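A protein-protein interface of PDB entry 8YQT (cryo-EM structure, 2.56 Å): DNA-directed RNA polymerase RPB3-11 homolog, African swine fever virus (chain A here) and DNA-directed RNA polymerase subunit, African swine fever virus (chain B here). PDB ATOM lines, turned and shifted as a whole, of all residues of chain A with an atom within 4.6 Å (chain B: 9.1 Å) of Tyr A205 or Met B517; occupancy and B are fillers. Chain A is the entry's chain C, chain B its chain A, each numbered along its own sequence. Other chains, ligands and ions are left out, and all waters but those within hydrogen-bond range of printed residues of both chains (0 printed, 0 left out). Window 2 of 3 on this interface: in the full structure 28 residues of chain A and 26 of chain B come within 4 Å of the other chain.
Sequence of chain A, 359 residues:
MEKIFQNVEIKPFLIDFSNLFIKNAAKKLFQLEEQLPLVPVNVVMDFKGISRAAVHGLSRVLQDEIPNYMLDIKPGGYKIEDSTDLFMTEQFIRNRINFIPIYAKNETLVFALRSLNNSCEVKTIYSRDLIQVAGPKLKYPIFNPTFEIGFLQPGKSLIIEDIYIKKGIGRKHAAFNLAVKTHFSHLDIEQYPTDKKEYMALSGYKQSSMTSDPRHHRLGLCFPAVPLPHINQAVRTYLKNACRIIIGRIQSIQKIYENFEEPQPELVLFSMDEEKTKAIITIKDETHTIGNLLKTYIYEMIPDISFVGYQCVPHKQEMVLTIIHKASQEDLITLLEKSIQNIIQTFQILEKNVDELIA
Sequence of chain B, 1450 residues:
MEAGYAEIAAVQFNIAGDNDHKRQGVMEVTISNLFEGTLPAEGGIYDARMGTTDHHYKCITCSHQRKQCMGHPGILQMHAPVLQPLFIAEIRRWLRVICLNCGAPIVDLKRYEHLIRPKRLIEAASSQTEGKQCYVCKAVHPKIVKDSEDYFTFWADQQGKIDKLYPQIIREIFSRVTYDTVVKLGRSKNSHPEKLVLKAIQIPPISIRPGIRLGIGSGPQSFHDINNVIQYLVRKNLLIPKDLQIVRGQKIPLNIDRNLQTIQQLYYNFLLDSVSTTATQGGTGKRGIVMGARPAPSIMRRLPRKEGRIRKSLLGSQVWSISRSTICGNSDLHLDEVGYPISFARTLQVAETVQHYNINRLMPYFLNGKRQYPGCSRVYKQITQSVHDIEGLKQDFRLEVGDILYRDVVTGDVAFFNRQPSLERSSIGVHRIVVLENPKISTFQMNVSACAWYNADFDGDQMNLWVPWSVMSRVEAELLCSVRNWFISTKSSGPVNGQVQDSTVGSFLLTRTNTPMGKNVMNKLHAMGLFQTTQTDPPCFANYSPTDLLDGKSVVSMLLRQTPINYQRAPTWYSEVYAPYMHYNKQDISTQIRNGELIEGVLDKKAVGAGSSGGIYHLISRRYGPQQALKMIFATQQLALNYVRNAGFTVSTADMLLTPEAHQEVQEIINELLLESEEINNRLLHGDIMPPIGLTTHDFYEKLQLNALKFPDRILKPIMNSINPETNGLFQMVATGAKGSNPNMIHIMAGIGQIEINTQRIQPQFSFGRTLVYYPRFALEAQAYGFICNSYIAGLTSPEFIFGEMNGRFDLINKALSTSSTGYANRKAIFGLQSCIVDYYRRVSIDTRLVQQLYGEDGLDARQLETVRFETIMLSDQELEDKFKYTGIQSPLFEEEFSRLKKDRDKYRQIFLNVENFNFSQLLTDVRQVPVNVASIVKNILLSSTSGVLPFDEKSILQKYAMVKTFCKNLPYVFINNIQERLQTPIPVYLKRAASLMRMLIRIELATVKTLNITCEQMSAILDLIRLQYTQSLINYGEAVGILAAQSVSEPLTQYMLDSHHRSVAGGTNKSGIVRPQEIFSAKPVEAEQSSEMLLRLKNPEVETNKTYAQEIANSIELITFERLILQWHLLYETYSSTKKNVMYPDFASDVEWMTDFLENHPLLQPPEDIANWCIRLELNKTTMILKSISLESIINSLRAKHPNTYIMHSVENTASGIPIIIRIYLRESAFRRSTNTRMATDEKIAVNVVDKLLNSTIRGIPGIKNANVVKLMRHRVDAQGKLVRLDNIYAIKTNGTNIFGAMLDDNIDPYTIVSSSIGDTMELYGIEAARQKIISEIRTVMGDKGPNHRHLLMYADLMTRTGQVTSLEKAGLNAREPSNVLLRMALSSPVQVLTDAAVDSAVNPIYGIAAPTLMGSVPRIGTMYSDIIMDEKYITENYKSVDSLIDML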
ATOM      1  N   SER A 185       4.053 -39.380  -6.476  1.00  0.00           N
ATOM      2  CA  SER A 185       2.741 -38.787  -6.684  1.00  0.00           C
ATOM      3  C   SER A 185       1.853 -39.085  -5.488  1.00  0.00           C
ATOM      4  O   SER A 185       2.130 -39.986  -4.695  1.00  0.00           O
ATOM      5  CB  SER A 185       2.093 -39.299  -7.975  1.00  0.00           C
ATOM      6  OG  SER A 185       1.781 -40.675  -7.884  1.00  0.00           O
ATOM      7  N   HIS A 186       0.778 -38.310  -5.372  1.00  0.00           N
ATOM      8  CA  HIS A 186      -0.247 -38.515  -4.361  1.00  0.00           C
ATOM      9  C   HIS A 186      -1.503 -39.039  -5.037  1.00  0.00           C
ATOM     10  O   HIS A 186      -1.997 -38.432  -5.991  1.00  0.00           O
ATOM     11  CB  HIS A 186      -0.556 -37.219  -3.610  1.00  0.00           C
ATOM     12  CG  HIS A 186       0.654 -36.539  -3.053  1.00  0.00           C
ATOM     13  ND1 HIS A 186       1.456 -37.116  -2.093  1.00  0.00           N
ATOM     14  CD2 HIS A 186       1.195 -35.329  -3.318  1.00  0.00           C
ATOM     15  CE1 HIS A 186       2.443 -36.290  -1.795  1.00  0.00           C
ATOM     16  NE2 HIS A 186       2.306 -35.199  -2.522  1.00  0.00           N
ATOM     17  N   ILE A 189      -5.295 -37.024  -4.145  1.00  0.00           N
ATOM     18  CA  ILE A 189      -5.582 -35.678  -4.622  1.00  0.00           C
ATOM     19  C   ILE A 189      -5.906 -35.767  -6.106  1.00  0.00           C
ATOM     20  O   ILE A 189      -5.161 -36.388  -6.872  1.00  0.00           O
ATOM     21  CB  ILE A 189      -4.404 -34.717  -4.379  1.00  0.00           C
ATOM     22  CG1 ILE A 189      -4.002 -34.715  -2.907  1.00  0.00           C
ATOM     23  CG2 ILE A 189      -4.768 -33.310  -4.814  1.00  0.00           C
ATOM     24  CD1 ILE A 189      -2.750 -33.927  -2.629  1.00  0.00           C
ATOM     25  N   GLU A 190      -7.021 -35.162  -6.507  1.00  0.00           N
ATOM     26  CA  GLU A 190      -7.389 -35.136  -7.912  1.00  0.00           C
ATOM     27  C   GLU A 190      -6.457 -34.209  -8.689  1.00  0.00           C
ATOM     28  O   GLU A 190      -5.851 -33.288  -8.137  1.00  0.00           O
ATOM     29  CB  GLU A 190      -8.839 -34.687  -8.083  1.00  0.00           C
ATOM     30  CG  GLU A 190      -9.868 -35.580  -7.405  1.00  0.00           C
ATOM     31  CD  GLU A 190      -9.563 -37.058  -7.552  1.00  0.00           C
ATOM     32  OE1 GLU A 190      -8.905 -37.629  -6.655  1.00  0.00           O
ATOM     33  OE2 GLU A 190      -9.985 -37.656  -8.564  1.00  0.00           O
ATOM     34  N   GLN A 191      -6.347 -34.463  -9.991  1.00  0.00           N
ATOM     35  CA  GLN A 191      -5.445 -33.708 -10.845  1.00  0.00           C
ATOM     36  C   GLN A 191      -6.191 -33.145 -12.046  1.00  0.00           C
ATOM     37  O   GLN A 191      -7.127 -33.759 -12.563  1.00  0.00           O
ATOM     38  CB  GLN A 191      -4.279 -34.568 -11.339  1.00  0.00           C
ATOM     39  CG  GLN A 191      -3.462 -35.212 -10.242  1.00  0.00           C
ATOM     40  CD  GLN A 191      -2.101 -35.655 -10.725  1.00  0.00           C
ATOM     41  OE1 GLN A 191      -1.654 -35.264 -11.800  1.00  0.00           O
ATOM     42  NE2 GLN A 191      -1.436 -36.490  -9.939  1.00  0.00           N
ATOM     43  N   TYR A 192      -5.761 -31.964 -12.480  1.00  0.00           N
ATOM     44  CA  TYR A 192      -6.239 -31.365 -13.713  1.00  0.00           C
ATOM     45  C   TYR A 192      -5.590 -32.031 -14.919  1.00  0.00           C
ATOM     46  O   TYR A 192      -4.529 -32.648 -14.805  1.00  0.00           O
ATOM     47  CB  TYR A 192      -5.914 -29.876 -13.750  1.00  0.00           C
ATOM     48  CG  TYR A 192      -6.620 -29.023 -12.729  1.00  0.00           C
ATOM     49  CD1 TYR A 192      -7.994 -28.844 -12.773  1.00  0.00           C
ATOM     50  CD2 TYR A 192      -5.904 -28.363 -11.744  1.00  0.00           C
ATOM     51  CE1 TYR A 192      -8.636 -28.051 -11.846  1.00  0.00           C
ATOM     52  CE2 TYR A 192      -6.536 -27.568 -10.818  1.00  0.00           C
ATOM     53  CZ  TYR A 192      -7.901 -27.415 -10.871  1.00  0.00           C
ATOM     54  OH  TYR A 192      -8.531 -26.620  -9.944  1.00  0.00           O
ATOM     55  N   SER A 203       0.737 -26.857 -11.124  1.00  0.00           N
ATOM     56  CA  SER A 203       1.320 -28.176 -10.898  1.00  0.00           C
ATOM     57  C   SER A 203       0.420 -29.280 -11.433  1.00  0.00           C
ATOM     58  O   SER A 203       0.901 -30.228 -12.060  1.00  0.00           O
ATOM     59  CB  SER A 203       1.584 -28.386  -9.410  1.00  0.00           C
ATOM     60  OG  SER A 203       0.373 -28.551  -8.695  1.00  0.00           O
ATOM     61  N   GLY A 204      -0.882 -29.178 -11.197  1.00  0.00           N
ATOM     62  CA  GLY A 204      -1.805 -30.191 -11.661  1.00  0.00           C
ATOM     63  C   GLY A 204      -2.754 -30.674 -10.588  1.00  0.00           C
ATOM     64  O   GLY A 204      -3.896 -31.026 -10.881  1.00  0.00           O
ATOM     65  N   TYR A 205      -2.293 -30.695  -9.341  1.00  0.00           N
ATOM     66  CA  TYR A 205      -3.150 -31.091  -8.233  1.00  0.00           C
ATOM     67  C   TYR A 205      -4.238 -30.053  -8.007  1.00  0.00           C
ATOM     68  O   TYR A 205      -4.026 -28.855  -8.203  1.00  0.00           O
ATOM     69  CB  TYR A 205      -2.324 -31.280  -6.962  1.00  0.00           C
ATOM     70  CG  TYR A 205      -1.449 -32.509  -6.993  1.00  0.00           C
ATOM     71  CD1 TYR A 205      -2.007 -33.777  -7.019  1.00  0.00           C
ATOM     72  CD2 TYR A 205      -0.070 -32.403  -7.002  1.00  0.00           C
ATOM     73  CE1 TYR A 205      -1.218 -34.899  -7.049  1.00  0.00           C
ATOM     74  CE2 TYR A 205       0.725 -33.522  -7.030  1.00  0.00           C
ATOM     75  CZ  TYR A 205       0.146 -34.766  -7.056  1.00  0.00           C
ATOM     76  OH  TYR A 205       0.937 -35.886  -7.087  1.00  0.00           O
ATOM     77  N   LYS A 206      -5.415 -30.520  -7.604  1.00  0.00           N
ATOM     78  CA  LYS A 206      -6.553 -29.634  -7.408  1.00  0.00           C
ATOM     79  C   LYS A 206      -6.596 -29.013  -6.021  1.00  0.00           C
ATOM     80  O   LYS A 206      -7.489 -28.204  -5.754  1.00  0.00           O
ATOM     81  CB  LYS A 206      -7.854 -30.388  -7.682  1.00  0.00           C
ATOM     82  CG  LYS A 206      -8.093 -30.656  -9.151  1.00  0.00           C
ATOM     83  CD  LYS A 206      -9.438 -31.302  -9.385  1.00  0.00           C
ATOM     84  CE  LYS A 206      -9.636 -31.623 -10.851  1.00  0.00           C
ATOM     85  NZ  LYS A 206     -10.937 -32.300 -11.094  1.00  0.00           N
ATOM     86  N   GLN A 207      -5.667 -29.364  -5.140  1.00  0.00           N
ATOM     87  CA  GLN A 207      -5.538 -28.743  -3.832  1.00  0.00           C
ATOM     88  C   GLN A 207      -4.158 -28.120  -3.715  1.00  0.00           C
ATOM     89  O   GLN A 207      -3.163 -28.713  -4.138  1.00  0.00           O
ATOM     90  CB  GLN A 207      -5.741 -29.756  -2.705  1.00  0.00           C
ATOM     91  CG  GLN A 207      -7.070 -30.476  -2.742  1.00  0.00           C
ATOM     92  CD  GLN A 207      -7.158 -31.569  -1.703  1.00  0.00           C
ATOM     93  OE1 GLN A 207      -6.242 -31.754  -0.906  1.00  0.00           O
ATOM     94  NE2 GLN A 207      -8.255 -32.310  -1.712  1.00  0.00           N
ATOM     95  N   SER A 208      -4.104 -26.919  -3.152  1.00  0.00           N
ATOM     96  CA  SER A 208      -2.828 -26.263  -2.915  1.00  0.00           C
ATOM     97  C   SER A 208      -2.038 -27.013  -1.851  1.00  0.00           C
ATOM     98  O   SER A 208      -2.598 -27.564  -0.902  1.00  0.00           O
ATOM     99  CB  SER A 208      -3.046 -24.816  -2.485  1.00  0.00           C
ATOM    100  OG  SER A 208      -1.814 -24.152  -2.290  1.00  0.00           O
ATOM    101  N   ARG B 512      -0.832 -11.547  -1.638  1.00  0.00           N
ATOM    102  CA  ARG B 512      -1.837 -11.572  -2.690  1.00  0.00           C
ATOM    103  C   ARG B 512      -3.131 -12.192  -2.179  1.00  0.00           C
ATOM    104  O   ARG B 512      -3.114 -13.172  -1.435  1.00  0.00           O
ATOM    105  CB  ARG B 512      -1.281 -12.361  -3.874  1.00  0.00           C
ATOM    106  CG  ARG B 512      -2.217 -12.646  -4.997  1.00  0.00           C
ATOM    107  CD  ARG B 512      -1.502 -13.517  -6.008  1.00  0.00           C
ATOM    108  NE  ARG B 512      -0.843 -14.647  -5.368  1.00  0.00           N
ATOM    109  CZ  ARG B 512      -0.324 -15.680  -6.017  1.00  0.00           C
ATOM    110  NH1 ARG B 512      -0.377 -15.764  -7.336  1.00  0.00           N
ATOM    111  NH2 ARG B 512       0.257 -16.655  -5.326  1.00  0.00           N
ATOM    112  N   THR B 513      -4.260 -11.598  -2.564  1.00  0.00           N
ATOM    113  CA  THR B 513      -5.546 -12.032  -2.028  1.00  0.00           C
ATOM    114  C   THR B 513      -5.956 -13.396  -2.568  1.00  0.00           C
ATOM    115  O   THR B 513      -6.368 -14.275  -1.804  1.00  0.00           O
ATOM    116  CB  THR B 513      -6.627 -10.998  -2.341  1.00  0.00           C
ATOM    117  OG1 THR B 513      -6.273  -9.740  -1.758  1.00  0.00           O
ATOM    118  CG2 THR B 513      -7.959 -11.444  -1.781  1.00  0.00           C
ATOM    119  N   ASN B 514      -5.855 -13.592  -3.880  1.00  0.00           N
ATOM    120  CA  ASN B 514      -6.325 -14.810  -4.522  1.00  0.00           C
ATOM    121  C   ASN B 514      -5.183 -15.470  -5.271  1.00  0.00           C
ATOM    122  O   ASN B 514      -4.445 -14.806  -6.003  1.00  0.00           O
ATOM    123  CB  ASN B 514      -7.478 -14.532  -5.490  1.00  0.00           C
ATOM    124  CG  ASN B 514      -8.733 -14.070  -4.790  1.00  0.00           C
ATOM    125  OD1 ASN B 514      -9.144 -12.921  -4.927  1.00  0.00           O
ATOM    126  ND2 ASN B 514      -9.353 -14.964  -4.036  1.00  0.00           N
ATOM    127  N   THR B 515      -5.052 -16.762  -5.083  1.00  0.00           N
ATOM    128  CA  THR B 515      -4.183 -17.659  -5.822  1.00  0.00           C
ATOM    129  C   THR B 515      -4.979 -18.285  -6.971  1.00  0.00           C
ATOM    130  O   THR B 515      -6.208 -18.358  -6.904  1.00  0.00           O
ATOM    131  CB  THR B 515      -3.631 -18.722  -4.862  1.00  0.00           C
ATOM    132  OG1 THR B 515      -2.515 -18.181  -4.147  1.00  0.00           O
ATOM    133  CG2 THR B 515      -3.205 -20.009  -5.547  1.00  0.00           C
ATOM    134  N   PRO B 516      -4.313 -18.709  -8.063  1.00  0.00           N
ATOM    135  CA  PRO B 516      -5.036 -19.411  -9.135  1.00  0.00           C
ATOM    136  C   PRO B 516      -5.838 -20.620  -8.670  1.00  0.00           C
ATOM    137  O   PRO B 516      -6.569 -21.220  -9.461  1.00  0.00           O
ATOM    138  CB  PRO B 516      -3.911 -19.835 -10.083  1.00  0.00           C
ATOM    139  CG  PRO B 516      -2.887 -18.797  -9.910  1.00  0.00           C
ATOM    140  CD  PRO B 516      -2.947 -18.347  -8.480  1.00  0.00           C
ATOM    141  N   MET B 517      -5.709 -20.990  -7.401  1.00  0.00           N
ATOM    142  CA  MET B 517      -6.409 -22.125  -6.816  1.00  0.00           C
ATOM    143  C   MET B 517      -7.329 -21.687  -5.684  1.00  0.00           C
ATOM    144  O   MET B 517      -7.502 -22.395  -4.692  1.00  0.00           O
ATOM    145  CB  MET B 517      -5.411 -23.167  -6.322  1.00  0.00           C
ATOM    146  CG  MET B 517      -4.527 -23.708  -7.421  1.00  0.00           C
ATOM    147  SD  MET B 517      -4.934 -25.408  -7.816  1.00  0.00           S
ATOM    148  CE  MET B 517      -4.106 -26.215  -6.461  1.00  0.00           C
ATOM    149  N   GLY B 518      -7.934 -20.512  -5.823  1.00  0.00           N
ATOM    150  CA  GLY B 518      -8.858 -20.018  -4.823  1.00  0.00           C
ATOM    151  C   GLY B 518      -8.264 -18.968  -3.912  1.00  0.00           C
ATOM    152  O   GLY B 518      -7.339 -18.252  -4.301  1.00  0.00           O
ATOM    153  N   LYS B 519      -8.793 -18.862  -2.696  1.00  0.00           N
ATOM    154  CA  LYS B 519      -8.278 -17.893  -1.741  1.00  0.00           C
ATOM    155  C   LYS B 519      -6.860 -18.257  -1.324  1.00  0.00           C
ATOM    156  O   LYS B 519      -6.519 -19.432  -1.172  1.00  0.00           O
ATOM    157  CB  LYS B 519      -9.187 -17.819  -0.516  1.00  0.00           C
ATOM    158  CG  LYS B 519     -10.242 -16.728  -0.599  1.00  0.00           C
ATOM    159  CD  LYS B 519     -10.768 -16.342   0.775  1.00  0.00           C
ATOM    160  CE  LYS B 519      -9.636 -16.134   1.769  1.00  0.00           C
ATOM    161  NZ  LYS B 519      -9.177 -14.718   1.829  1.00  0.00           N
ATOM    162  N   ASN B 520      -6.030 -17.233  -1.145  1.00  0.00           N
ATOM    163  CA  ASN B 520      -4.632 -17.412  -0.763  1.00  0.00           C
ATOM    164  C   ASN B 520      -4.569 -17.626   0.746  1.00  0.00           C
ATOM    165  O   ASN B 520      -4.300 -16.715   1.532  1.00  0.00           O
ATOM    166  CB  ASN B 520      -3.808 -16.210  -1.200  1.00  0.00           C
ATOM    167  CG  ASN B 520      -2.326 -16.428  -1.044  1.00  0.00           C
ATOM    168  OD1 ASN B 520      -1.879 -17.517  -0.695  1.00  0.00           O
ATOM    169  ND2 ASN B 520      -1.550 -15.386  -1.298  1.00  0.00           N
ATOM    170  N   VAL B 521      -4.832 -18.864   1.155  1.00  0.00           N
ATOM    171  CA  VAL B 521      -4.817 -19.246   2.558  1.00  0.00           C
ATOM    172  C   VAL B 521      -3.916 -20.464   2.728  1.00  0.00           C
ATOM    173  O   VAL B 521      -3.566 -21.151   1.769  1.00  0.00           O
ATOM    174  CB  VAL B 521      -6.227 -19.532   3.111  1.00  0.00           C
ATOM    175  CG1 VAL B 521      -7.058 -18.268   3.122  1.00  0.00           C
ATOM    176  CG2 VAL B 521      -6.906 -20.617   2.301  1.00  0.00           C
ATOM    177  N   TYR B 643       7.325 -18.766   1.912  1.00  0.00           N
ATOM    178  CA  TYR B 643       6.082 -18.896   1.165  1.00  0.00           C
ATOM    179  C   TYR B 643       6.342 -19.426  -0.238  1.00  0.00           C
ATOM    180  O   TYR B 643       5.660 -20.344  -0.702  1.00  0.00           O
ATOM    181  CB  TYR B 643       5.362 -17.550   1.102  1.00  0.00           C
ATOM    182  CG  TYR B 643       4.037 -17.626   0.389  1.00  0.00           C
ATOM    183  CD1 TYR B 643       2.886 -17.984   1.068  1.00  0.00           C
ATOM    184  CD2 TYR B 643       3.941 -17.363  -0.967  1.00  0.00           C
ATOM    185  CE1 TYR B 643       1.679 -18.065   0.421  1.00  0.00           C
ATOM    186  CE2 TYR B 643       2.739 -17.447  -1.621  1.00  0.00           C
ATOM    187  CZ  TYR B 643       1.613 -17.798  -0.924  1.00  0.00           C
ATOM    188  OH  TYR B 643       0.410 -17.878  -1.575  1.00  0.00           O
ATOM    189  N   ALA B 647       4.907 -22.237  -2.759  1.00  0.00           N
ATOM    190  CA  ALA B 647       4.090 -21.740  -3.857  1.00  0.00           C
ATOM    191  C   ALA B 647       4.781 -21.921  -5.201  1.00  0.00           C
ATOM    192  O   ALA B 647       4.125 -22.218  -6.203  1.00  0.00           O
ATOM    193  CB  ALA B 647       3.752 -20.268  -3.635  1.00  0.00           C
ATOM    194  N   GLU B 726      -2.079 -13.633 -13.356  1.00  0.00           N
ATOM    195  CA  GLU B 726      -2.120 -14.446 -12.151  1.00  0.00           C
ATOM    196  C   GLU B 726      -1.029 -15.506 -12.128  1.00  0.00           C
ATOM    197  O   GLU B 726      -0.659 -15.967 -11.045  1.00  0.00           O
ATOM    198  CB  GLU B 726      -3.490 -15.108 -12.024  1.00  0.00           C
ATOM    199  CG  GLU B 726      -4.381 -14.493 -10.967  1.00  0.00           C
ATOM    200  CD  GLU B 726      -5.420 -15.465 -10.446  1.00  0.00           C
ATOM    201  OE1 GLU B 726      -6.004 -15.199  -9.375  1.00  0.00           O
ATOM    202  OE2 GLU B 726      -5.655 -16.495 -11.112  1.00  0.00           O
ATOM    203  N   THR B 727      -0.508 -15.905 -13.287  1.00  0.00           N
ATOM    204  CA  THR B 727       0.464 -16.986 -13.358  1.00  0.00           C
ATOM    205  C   THR B 727       1.750 -16.644 -14.092  1.00  0.00           C
ATOM    206  O   THR B 727       2.742 -17.356 -13.901  1.00  0.00           O
ATOM    207  CB  THR B 727      -0.152 -18.227 -14.026  1.00  0.00           C
ATOM    208  OG1 THR B 727      -0.482 -17.925 -15.385  1.00  0.00           O
ATOM    209  CG2 THR B 727      -1.402 -18.671 -13.295  1.00  0.00           C
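Of the 14 printed residues of chain B, 1 touches a printed residue of chain A. Printed residues of chain B that touch a printed residue of chain A: Met B517. Of the 12 printed residues of chain A, 4 touch a printed residue of chain B. Among the printed residues, 4 pairs touch across the chains. Among the printed residues, no Asp or Glu carboxylate lies within 4 Å of a Lys or Arg side-chain nitrogen of the other chain.
No residue of chain B comes within 4 Å of Ser A185. No residue of chain B comes within 4 Å of Gly A204. Of chain B, only Met B517 (3.2 Å) comes within 4 Å of Tyr A205. Printed residues of chain B within 4 Å of Lys A206: Met B517 (3.8 Å). Of the printed residues of chain B, Gln A207 touches Met B517. Of the printed residues of chain B, Ser A208 touches Met B517. Met B517 touches just these residues of chain A: Tyr A205 (3.2 Å), Lys A206 (3.8 Å), Gln A207 (3.3 Å) and Ser A208 (3.4 Å). The nearest residue of chain B that does not touch Tyr A205 is Pro B516 (8.1 Å). The nearest printed residue of chain B that does not touch Ser A208 is Val B521 (5.3 Å).
Among the printed residues, pairs that only touch across the chains: Gln A207 with Met B517, Ser A208 with Met B517 and Lys A206 with Met B517.
O of Tyr A205 sits close to SD of Met B517 (3.6 Å).
O of Glu A190 sits at hydrogen-bond distance from N of Lys A206. OG of Ser A203 is in hydrogen-bond range of N of Tyr A205 (3.5 Å). The backbone NH (N) of His A186 sits at hydrogen-bond distance from the side-chain hydroxyl (OH) of Tyr A205 (3.0 Å).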
